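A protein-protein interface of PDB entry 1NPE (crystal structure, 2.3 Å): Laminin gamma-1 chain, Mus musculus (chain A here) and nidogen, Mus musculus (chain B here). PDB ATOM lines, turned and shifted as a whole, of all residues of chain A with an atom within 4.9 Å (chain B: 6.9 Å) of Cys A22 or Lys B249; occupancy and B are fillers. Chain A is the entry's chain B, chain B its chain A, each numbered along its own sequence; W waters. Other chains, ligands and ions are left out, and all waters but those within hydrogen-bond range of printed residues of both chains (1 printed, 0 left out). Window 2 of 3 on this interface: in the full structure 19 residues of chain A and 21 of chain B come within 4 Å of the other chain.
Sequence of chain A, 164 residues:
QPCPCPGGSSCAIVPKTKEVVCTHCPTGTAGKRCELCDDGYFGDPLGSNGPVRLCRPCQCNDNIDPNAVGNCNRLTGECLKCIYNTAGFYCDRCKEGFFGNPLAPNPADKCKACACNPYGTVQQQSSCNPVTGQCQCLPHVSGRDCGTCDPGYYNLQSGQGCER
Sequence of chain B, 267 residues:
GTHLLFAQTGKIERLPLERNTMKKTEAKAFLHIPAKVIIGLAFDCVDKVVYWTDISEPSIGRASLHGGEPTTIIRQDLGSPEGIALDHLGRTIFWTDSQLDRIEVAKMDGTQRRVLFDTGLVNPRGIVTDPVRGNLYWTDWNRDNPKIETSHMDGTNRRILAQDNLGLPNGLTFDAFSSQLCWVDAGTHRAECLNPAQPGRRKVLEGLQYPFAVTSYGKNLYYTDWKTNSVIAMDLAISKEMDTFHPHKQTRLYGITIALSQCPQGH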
ATOM      1  N   PRO A   4       9.855  10.215 -37.453  1.00  0.00           N
ATOM      2  CA  PRO A   4      11.038  10.914 -36.937  1.00  0.00           C
ATOM      3  C   PRO A   4      11.251  10.495 -35.482  1.00  0.00           C
ATOM      4  O   PRO A   4      11.107  11.304 -34.564  1.00  0.00           O
ATOM      5  CB  PRO A   4      10.632  12.384 -37.051  1.00  0.00           C
ATOM      6  CG  PRO A   4       9.162  12.338 -36.777  1.00  0.00           C
ATOM      7  CD  PRO A   4       8.715  11.140 -37.591  1.00  0.00           C
ATOM      8  N   CYS A   5      11.598   9.224 -35.294  1.00  0.00           N
ATOM      9  CA  CYS A   5      11.795   8.649 -33.969  1.00  0.00           C
ATOM     10  C   CYS A   5      12.951   7.668 -33.936  1.00  0.00           C
ATOM     11  O   CYS A   5      13.243   7.001 -34.927  1.00  0.00           O
ATOM     12  CB  CYS A   5      10.533   7.898 -33.546  1.00  0.00           C
ATOM     13  SG  CYS A   5       9.025   8.907 -33.587  1.00  0.00           S
ATOM     14  N   PRO A   6      13.618   7.552 -32.780  1.00  0.00           N
ATOM     15  CA  PRO A   6      14.747   6.627 -32.641  1.00  0.00           C
ATOM     16  C   PRO A   6      14.280   5.178 -32.519  1.00  0.00           C
ATOM     17  O   PRO A   6      13.088   4.913 -32.357  1.00  0.00           O
ATOM     18  CB  PRO A   6      15.410   7.094 -31.340  1.00  0.00           C
ATOM     19  CG  PRO A   6      15.012   8.549 -31.243  1.00  0.00           C
ATOM     20  CD  PRO A   6      13.563   8.480 -31.638  1.00  0.00           C
ATOM     21  N   SER A   9      10.834   2.962 -33.668  1.00  0.00           N
ATOM     22  CA  SER A   9       9.569   3.139 -32.979  1.00  0.00           C
ATOM     23  C   SER A   9       8.508   3.646 -33.942  1.00  0.00           C
ATOM     24  O   SER A   9       8.795   4.423 -34.858  1.00  0.00           O
ATOM     25  CB  SER A   9       9.723   4.127 -31.818  1.00  0.00           C
ATOM     26  OG  SER A   9       8.460   4.465 -31.258  1.00  0.00           O
ATOM     27  N   SER A  10       7.282   3.184 -33.742  1.00  0.00           N
ATOM     28  CA  SER A  10       6.168   3.634 -34.560  1.00  0.00           C
ATOM     29  C   SER A  10       5.788   5.020 -34.032  1.00  0.00           C
ATOM     30  O   SER A  10       6.205   5.412 -32.938  1.00  0.00           O
ATOM     31  CB  SER A  10       4.990   2.677 -34.413  1.00  0.00           C
ATOM     32  OG  SER A  10       4.542   2.638 -33.070  1.00  0.00           O
ATOM     33  N   CYS A  11       4.995   5.758 -34.797  1.00  0.00           N
ATOM     34  CA  CYS A  11       4.591   7.090 -34.370  1.00  0.00           C
ATOM     35  C   CYS A  11       3.171   7.430 -34.777  1.00  0.00           C
ATOM     36  O   CYS A  11       2.568   6.761 -35.616  1.00  0.00           O
ATOM     37  CB  CYS A  11       5.536   8.138 -34.950  1.00  0.00           C
ATOM     38  SG  CYS A  11       5.466   8.273 -36.763  1.00  0.00           S
ATOM     39  N   VAL A  20       3.437  15.290 -33.702  1.00  0.00           N
ATOM     40  CA  VAL A  20       3.819  13.904 -33.904  1.00  0.00           C
ATOM     41  C   VAL A  20       4.318  13.334 -32.588  1.00  0.00           C
ATOM     42  O   VAL A  20       5.069  13.972 -31.854  1.00  0.00           O
ATOM     43  CB  VAL A  20       4.867  13.722 -35.054  1.00  0.00           C
ATOM     44  CG1 VAL A  20       5.166  15.048 -35.710  1.00  0.00           C
ATOM     45  CG2 VAL A  20       6.130  13.049 -34.554  1.00  0.00           C
ATOM     46  N   VAL A  21       3.876  12.124 -32.296  1.00  0.00           N
ATOM     47  CA  VAL A  21       4.242  11.454 -31.069  1.00  0.00           C
ATOM     48  C   VAL A  21       4.896  10.095 -31.339  1.00  0.00           C
ATOM     49  O   VAL A  21       4.323   9.250 -32.028  1.00  0.00           O
ATOM     50  CB  VAL A  21       2.981  11.226 -30.186  1.00  0.00           C
ATOM     51  CG1 VAL A  21       3.370  10.691 -28.831  1.00  0.00           C
ATOM     52  CG2 VAL A  21       2.194  12.518 -30.037  1.00  0.00           C
ATOM     53  N   CYS A  22       6.117   9.909 -30.843  1.00  0.00           N
ATOM     54  CA  CYS A  22       6.798   8.629 -30.983  1.00  0.00           C
ATOM     55  C   CYS A  22       6.164   7.727 -29.938  1.00  0.00           C
ATOM     56  O   CYS A  22       5.911   8.164 -28.817  1.00  0.00           O
ATOM     57  CB  CYS A  22       8.286   8.776 -30.690  1.00  0.00           C
ATOM     58  SG  CYS A  22       9.109   9.917 -31.827  1.00  0.00           S
ATOM     59  N   THR A  23       5.890   6.480 -30.298  1.00  0.00           N
ATOM     60  CA  THR A  23       5.272   5.558 -29.355  1.00  0.00           C
ATOM     61  C   THR A  23       6.235   5.215 -28.227  1.00  0.00           C
ATOM     62  O   THR A  23       5.875   5.279 -27.043  1.00  0.00           O
ATOM     63  CB  THR A  23       4.778   4.271 -30.057  1.00  0.00           C
ATOM     64  OG1 THR A  23       3.785   4.619 -31.032  1.00  0.00           O
ATOM     65  CG2 THR A  23       4.148   3.310 -29.052  1.00  0.00           C
ATOM     66  N   HIS A  24       7.465   4.886 -28.608  1.00  0.00           N
ATOM     67  CA  HIS A  24       8.513   4.528 -27.664  1.00  0.00           C
ATOM     68  C   HIS A  24       9.652   5.546 -27.707  1.00  0.00           C
ATOM     69  O   HIS A  24       9.791   6.309 -28.667  1.00  0.00           O
ATOM     70  CB  HIS A  24       9.065   3.140 -28.000  1.00  0.00           C
ATOM     71  CG  HIS A  24       8.034   2.053 -27.961  1.00  0.00           C
ATOM     72  ND1 HIS A  24       7.181   1.797 -29.012  1.00  0.00           N
ATOM     73  CD2 HIS A  24       7.717   1.159 -26.994  1.00  0.00           C
ATOM     74  CE1 HIS A  24       6.381   0.794 -28.695  1.00  0.00           C
ATOM     75  NE2 HIS A  24       6.686   0.388 -27.476  1.00  0.00           N
ATOM     76  N   CYS A  25      10.454   5.562 -26.649  1.00  0.00           N
ATOM     77  CA  CYS A  25      11.599   6.458 -26.551  1.00  0.00           C
ATOM     78  C   CYS A  25      12.745   5.721 -25.901  1.00  0.00           C
ATOM     79  O   CYS A  25      12.537   4.827 -25.087  1.00  0.00           O
ATOM     80  CB  CYS A  25      11.271   7.706 -25.729  1.00  0.00           C
ATOM     81  SG  CYS A  25      10.382   9.005 -26.645  1.00  0.00           S
ATOM     82  N   GLY A  31       9.357  13.067 -23.626  1.00  0.00           N
ATOM     83  CA  GLY A  31       8.756  13.996 -24.564  1.00  0.00           C
ATOM     84  C   GLY A  31       8.139  13.294 -25.760  1.00  0.00           C
ATOM     85  O   GLY A  31       8.408  12.120 -26.007  1.00  0.00           O
ATOM     86  N   LYS A  32       7.324  14.025 -26.511  1.00  0.00           N
ATOM     87  CA  LYS A  32       6.650  13.486 -27.685  1.00  0.00           C
ATOM     88  C   LYS A  32       7.596  12.921 -28.745  1.00  0.00           C
ATOM     89  O   LYS A  32       7.323  11.869 -29.322  1.00  0.00           O
ATOM     90  CB  LYS A  32       5.723  14.543 -28.290  1.00  0.00           C
ATOM     91  CG  LYS A  32       4.543  14.892 -27.390  1.00  0.00           C
ATOM     92  CD  LYS A  32       3.748  16.077 -27.922  1.00  0.00           C
ATOM     93  CE  LYS A  32       4.555  17.362 -27.866  1.00  0.00           C
ATOM     94  NZ  LYS A  32       3.782  18.507 -28.418  1.00  0.00           N
ATOM     95  N   ARG A  33       8.710  13.609 -28.989  1.00  0.00           N
ATOM     96  CA  ARG A  33       9.685  13.152 -29.975  1.00  0.00           C
ATOM     97  C   ARG A  33      10.981  12.680 -29.312  1.00  0.00           C
ATOM     98  O   ARG A  33      12.018  12.573 -29.971  1.00  0.00           O
ATOM     99  CB  ARG A  33      10.016  14.271 -30.965  1.00  0.00           C
ATOM    100  CG  ARG A  33       8.841  14.800 -31.777  1.00  0.00           C
ATOM    101  CD  ARG A  33       9.335  15.341 -33.113  1.00  0.00           C
ATOM    102  NE  ARG A  33       8.328  16.140 -33.810  1.00  0.00           N
ATOM    103  CZ  ARG A  33       8.461  16.598 -35.055  1.00  0.00           C
ATOM    104  NH1 ARG A  33       9.557  16.328 -35.760  1.00  0.00           N
ATOM    105  NH2 ARG A  33       7.520  17.379 -35.575  1.00  0.00           N
ATOM    106  N   CYS A  34      10.914  12.372 -28.018  1.00  0.00           N
ATOM    107  CA  CYS A  34      12.092  11.958 -27.250  1.00  0.00           C
ATOM    108  C   CYS A  34      13.131  13.080 -27.377  1.00  0.00           C
ATOM    109  O   CYS A  34      14.337  12.827 -27.393  1.00  0.00           O
ATOM    110  CB  CYS A  34      12.694  10.649 -27.784  1.00  0.00           C
ATOM    111  SG  CYS A  34      11.523   9.356 -28.287  1.00  0.00           S
ATOM    112  N   GLN B   8       3.925  11.718 -15.769  1.00  0.00           N
ATOM    113  CA  GLN B   8       5.180  11.331 -16.407  1.00  0.00           C
ATOM    114  C   GLN B   8       5.835  12.643 -16.805  1.00  0.00           C
ATOM    115  O   GLN B   8       5.198  13.702 -16.738  1.00  0.00           O
ATOM    116  CB  GLN B   8       4.952  10.481 -17.657  1.00  0.00           C
ATOM    117  CG  GLN B   8       4.899   8.988 -17.397  1.00  0.00           C
ATOM    118  CD  GLN B   8       4.662   8.173 -18.660  1.00  0.00           C
ATOM    119  OE1 GLN B   8       3.811   8.511 -19.479  1.00  0.00           O
ATOM    120  NE2 GLN B   8       5.406   7.085 -18.813  1.00  0.00           N
ATOM    121  N   LYS B  11       3.983  15.172 -19.379  1.00  0.00           N
ATOM    122  CA  LYS B  11       2.584  14.816 -19.631  1.00  0.00           C
ATOM    123  C   LYS B  11       1.836  14.237 -18.436  1.00  0.00           C
ATOM    124  O   LYS B  11       2.417  13.963 -17.390  1.00  0.00           O
ATOM    125  CB  LYS B  11       2.517  13.782 -20.761  1.00  0.00           C
ATOM    126  CG  LYS B  11       3.362  12.544 -20.489  1.00  0.00           C
ATOM    127  CD  LYS B  11       3.240  11.495 -21.588  1.00  0.00           C
ATOM    128  CE  LYS B  11       1.867  10.850 -21.589  1.00  0.00           C
ATOM    129  NZ  LYS B  11       1.814   9.759 -22.592  1.00  0.00           N
ATOM    130  N   HIS B  32      -0.508  17.384 -22.567  1.00  0.00           N
ATOM    131  CA  HIS B  32       0.911  17.424 -22.872  1.00  0.00           C
ATOM    132  C   HIS B  32       1.456  18.790 -22.458  1.00  0.00           C
ATOM    133  O   HIS B  32       0.981  19.829 -22.932  1.00  0.00           O
ATOM    134  CB  HIS B  32       1.164  17.228 -24.371  1.00  0.00           C
ATOM    135  CG  HIS B  32       1.269  15.797 -24.788  1.00  0.00           C
ATOM    136  ND1 HIS B  32       0.343  15.193 -25.611  1.00  0.00           N
ATOM    137  CD2 HIS B  32       2.206  14.858 -24.524  1.00  0.00           C
ATOM    138  CE1 HIS B  32       0.706  13.945 -25.839  1.00  0.00           C
ATOM    139  NE2 HIS B  32       1.834  13.716 -25.190  1.00  0.00           N
ATOM    140  N   ASN B 229       8.280   0.528 -13.777  1.00  0.00           N
ATOM    141  CA  ASN B 229       7.733   1.490 -14.731  1.00  0.00           C
ATOM    142  C   ASN B 229       6.291   1.148 -15.080  1.00  0.00           C
ATOM    143  O   ASN B 229       5.930   1.057 -16.249  1.00  0.00           O
ATOM    144  CB  ASN B 229       8.585   1.552 -16.000  1.00  0.00           C
ATOM    145  CG  ASN B 229       9.817   2.412 -15.827  1.00  0.00           C
ATOM    146  OD1 ASN B 229       9.722   3.580 -15.443  1.00  0.00           O
ATOM    147  ND2 ASN B 229      10.983   1.842 -16.102  1.00  0.00           N
ATOM    148  N   HIS B 246       1.698  -1.199 -18.148  1.00  0.00           N
ATOM    149  CA  HIS B 246       2.981  -0.678 -18.593  1.00  0.00           C
ATOM    150  C   HIS B 246       2.742   0.268 -19.754  1.00  0.00           C
ATOM    151  O   HIS B 246       2.370  -0.180 -20.840  1.00  0.00           O
ATOM    152  CB  HIS B 246       3.891  -1.791 -19.127  1.00  0.00           C
ATOM    153  CG  HIS B 246       4.384  -2.745 -18.090  1.00  0.00           C
ATOM    154  ND1 HIS B 246       3.584  -3.723 -17.539  1.00  0.00           N
ATOM    155  CD2 HIS B 246       5.614  -2.917 -17.550  1.00  0.00           C
ATOM    156  CE1 HIS B 246       4.301  -4.456 -16.707  1.00  0.00           C
ATOM    157  NE2 HIS B 246       5.536  -3.990 -16.696  1.00  0.00           N
ATOM    158  N   PRO B 247       2.882   1.586 -19.539  1.00  0.00           N
ATOM    159  CA  PRO B 247       2.672   2.506 -20.662  1.00  0.00           C
ATOM    160  C   PRO B 247       3.790   2.254 -21.684  1.00  0.00           C
ATOM    161  O   PRO B 247       4.915   1.946 -21.298  1.00  0.00           O
ATOM    162  CB  PRO B 247       2.808   3.880 -20.010  1.00  0.00           C
ATOM    163  CG  PRO B 247       3.667   3.624 -18.806  1.00  0.00           C
ATOM    164  CD  PRO B 247       3.133   2.322 -18.290  1.00  0.00           C
ATOM    165  N   HIS B 248       3.473   2.340 -22.974  1.00  0.00           N
ATOM    166  CA  HIS B 248       4.467   2.093 -24.023  1.00  0.00           C
ATOM    167  C   HIS B 248       5.752   2.912 -23.869  1.00  0.00           C
ATOM    168  O   HIS B 248       6.852   2.389 -24.051  1.00  0.00           O
ATOM    169  CB  HIS B 248       3.854   2.286 -25.414  1.00  0.00           C
ATOM    170  CG  HIS B 248       2.884   1.210 -25.793  1.00  0.00           C
ATOM    171  ND1 HIS B 248       3.261  -0.107 -25.947  1.00  0.00           N
ATOM    172  CD2 HIS B 248       1.543   1.242 -25.979  1.00  0.00           C
ATOM    173  CE1 HIS B 248       2.193  -0.841 -26.201  1.00  0.00           C
ATOM    174  NE2 HIS B 248       1.138  -0.047 -26.228  1.00  0.00           N
ATOM    175  N   LYS B 249       5.601   4.187 -23.528  1.00  0.00           N
ATOM    176  CA  LYS B 249       6.740   5.074 -23.319  1.00  0.00           C
ATOM    177  C   LYS B 249       7.175   4.842 -21.868  1.00  0.00           C
ATOM    178  O   LYS B 249       6.602   5.416 -20.938  1.00  0.00           O
ATOM    179  CB  LYS B 249       6.313   6.529 -23.536  1.00  0.00           C
ATOM    180  CG  LYS B 249       7.447   7.522 -23.480  1.00  0.00           C
ATOM    181  CD  LYS B 249       7.761   8.073 -24.840  1.00  0.00           C
ATOM    182  CE  LYS B 249       6.634   8.926 -25.367  1.00  0.00           C
ATOM    183  NZ  LYS B 249       6.973   9.521 -26.686  1.00  0.00           N
ATOM    184  N   GLN B 250       8.174   3.981 -21.687  1.00  0.00           N
ATOM    185  CA  GLN B 250       8.660   3.604 -20.358  1.00  0.00           C
ATOM    186  C   GLN B 250       9.483   4.628 -19.563  1.00  0.00           C
ATOM    187  O   GLN B 250      10.572   4.319 -19.080  1.00  0.00           O
ATOM    188  CB  GLN B 250       9.390   2.247 -20.437  1.00  0.00           C
ATOM    189  CG  GLN B 250       8.521   1.095 -20.996  1.00  0.00           C
ATOM    190  CD  GLN B 250       9.257  -0.250 -21.099  1.00  0.00           C
ATOM    191  OE1 GLN B 250      10.333  -0.348 -21.703  1.00  0.00           O
ATOM    192  NE2 GLN B 250       8.659  -1.300 -20.528  1.00  0.00           N
ATOM    193  N   THR B 251       8.956   5.843 -19.415  1.00  0.00           N
ATOM    194  CA  THR B 251       9.645   6.875 -18.640  1.00  0.00           C
ATOM    195  C   THR B 251       9.148   6.834 -17.183  1.00  0.00           C
ATOM    196  O   THR B 251       8.174   6.151 -16.870  1.00  0.00           O
ATOM    197  CB  THR B 251       9.452   8.296 -19.243  1.00  0.00           C
ATOM    198  OG1 THR B 251       8.081   8.694 -19.140  1.00  0.00           O
ATOM    199  CG2 THR B 251       9.859   8.320 -20.704  1.00  0.00           C
ATOM    200  N   ARG B 252       9.844   7.537 -16.296  1.00  0.00           N
ATOM    201  CA  ARG B 252       9.509   7.570 -14.872  1.00  0.00           C
ATOM    202  C   ARG B 252       8.073   8.034 -14.575  1.00  0.00           C
ATOM    203  O   ARG B 252       7.656   9.112 -14.998  1.00  0.00           O
ATOM    204  CB  ARG B 252      10.494   8.484 -14.142  1.00  0.00           C
ATOM    205  CG  ARG B 252      10.689   8.179 -12.670  1.00  0.00           C
ATOM    206  CD  ARG B 252      11.547   6.957 -12.490  1.00  0.00           C
ATOM    207  NE  ARG B 252      12.719   7.219 -11.664  1.00  0.00           N
ATOM    208  CZ  ARG B 252      13.657   6.315 -11.393  1.00  0.00           C
ATOM    209  NH1 ARG B 252      13.562   5.085 -11.881  1.00  0.00           N
ATOM    210  NH2 ARG B 252      14.694   6.641 -10.637  1.00  0.00           N
ATOM    211  N   LEU B 253       7.317   7.193 -13.880  1.00  0.00           N
ATOM    212  CA  LEU B 253       5.947   7.516 -13.497  1.00  0.00           C
ATOM    213  C   LEU B 253       5.959   8.268 -12.166  1.00  0.00           C
ATOM    214  O   LEU B 253       6.751   7.945 -11.289  1.00  0.00           O
ATOM    215  CB  LEU B 253       5.125   6.236 -13.324  1.00  0.00           C
ATOM    216  CG  LEU B 253       4.916   5.312 -14.525  1.00  0.00           C
ATOM    217  CD1 LEU B 253       3.882   4.274 -14.151  1.00  0.00           C
ATOM    218  CD2 LEU B 253       4.415   6.103 -15.707  1.00  0.00           C
HETATM  219  O   HOH W   1       9.570   3.462 -24.581  1.00  0.00           O
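SG of Cys A25 lies close to NZ of Lys B249, at 3.4 Å. The backbone carbonyl oxygen of Cys A22 sits at hydrogen-bond distance from the side-chain amino group of Lys B249 (2.7 Å). The side-chain amino group of Lys B249 is in hydrogen-bond range of the backbone carbonyl oxygen of Gly A31.
SG of Cys A25 is disulfide-bonded to SG of Cys A34. The backbone NH (N) of Thr A23 is in hydrogen-bond range of the side-chain hydroxyl (OG) of Ser A9. The side-chain sulfur (SG) of Cys A5 is disulfide-bonded to the side-chain sulfur (SG) of Cys A22 (2.0 Å). The backbone NH (N) of His A24 is in hydrogen-bond range of the side-chain hydroxyl (OG) of Ser A9. The backbone carbonyl oxygen (O) of Lys B249 is in hydrogen-bond range of the side-chain amide nitrogen (NE2) of Gln B8 (3.0 Å). The backbone carbonyl oxygen (O) of Lys A32 is in hydrogen-bond range of the backbone NH (N) of Cys A22, 2.8 Å away.
Among the printed residues, pairs that only touch across the chains: Thr A23 with His B248 (3.8 Å), Thr A23 with Lys B249 (3.7 Å), His A24 with His B248 (3.3 Å), Lys A32 with His B32 (3.7 Å) and Lys A32 with Lys B249 (3.5 Å).
Of chain B, only Lys B249 (2.7 Å) comes within 4 Å of Cys A22. Of the printed residues of chain B, Thr A23 touches His B248 and Lys B249. Printed residues of chain B within 4 Å of His A24: His B248 (3.3 Å). Printed residues of chain B within 4 Å of Cys A25: Lys B249 (3.3 Å). Of chain A, only Cys A22 (2.7 Å), Thr A23 (3.7 Å), Cys A25 (3.3 Å), Gly A31 (3.0 Å) and Lys A32 (3.5 Å) come within 4 Å of Lys B249. The nearest printed residue of chain B that does not touch Cys A22 is His B248 (7.1 Å). The nearest printed residue of chain B that does not touch His A24 is Lys B249 (4.3 Å).
Of the 16 printed residues of chain A, 6 touch a printed residue of chain B. Among the printed residues, 8 pairs touch across the chains. Among the printed residues, no Asp or Glu carboxylate lies within 4 Å of a Lys or Arg side-chain nitrogen of the other chain.
Water W1 lies within hydrogen-bond range of the backbone carbonyl oxygen (O) of His B248, the backbone NH (N) of Cys A25 and the backbone NH (N) of Gln B250.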
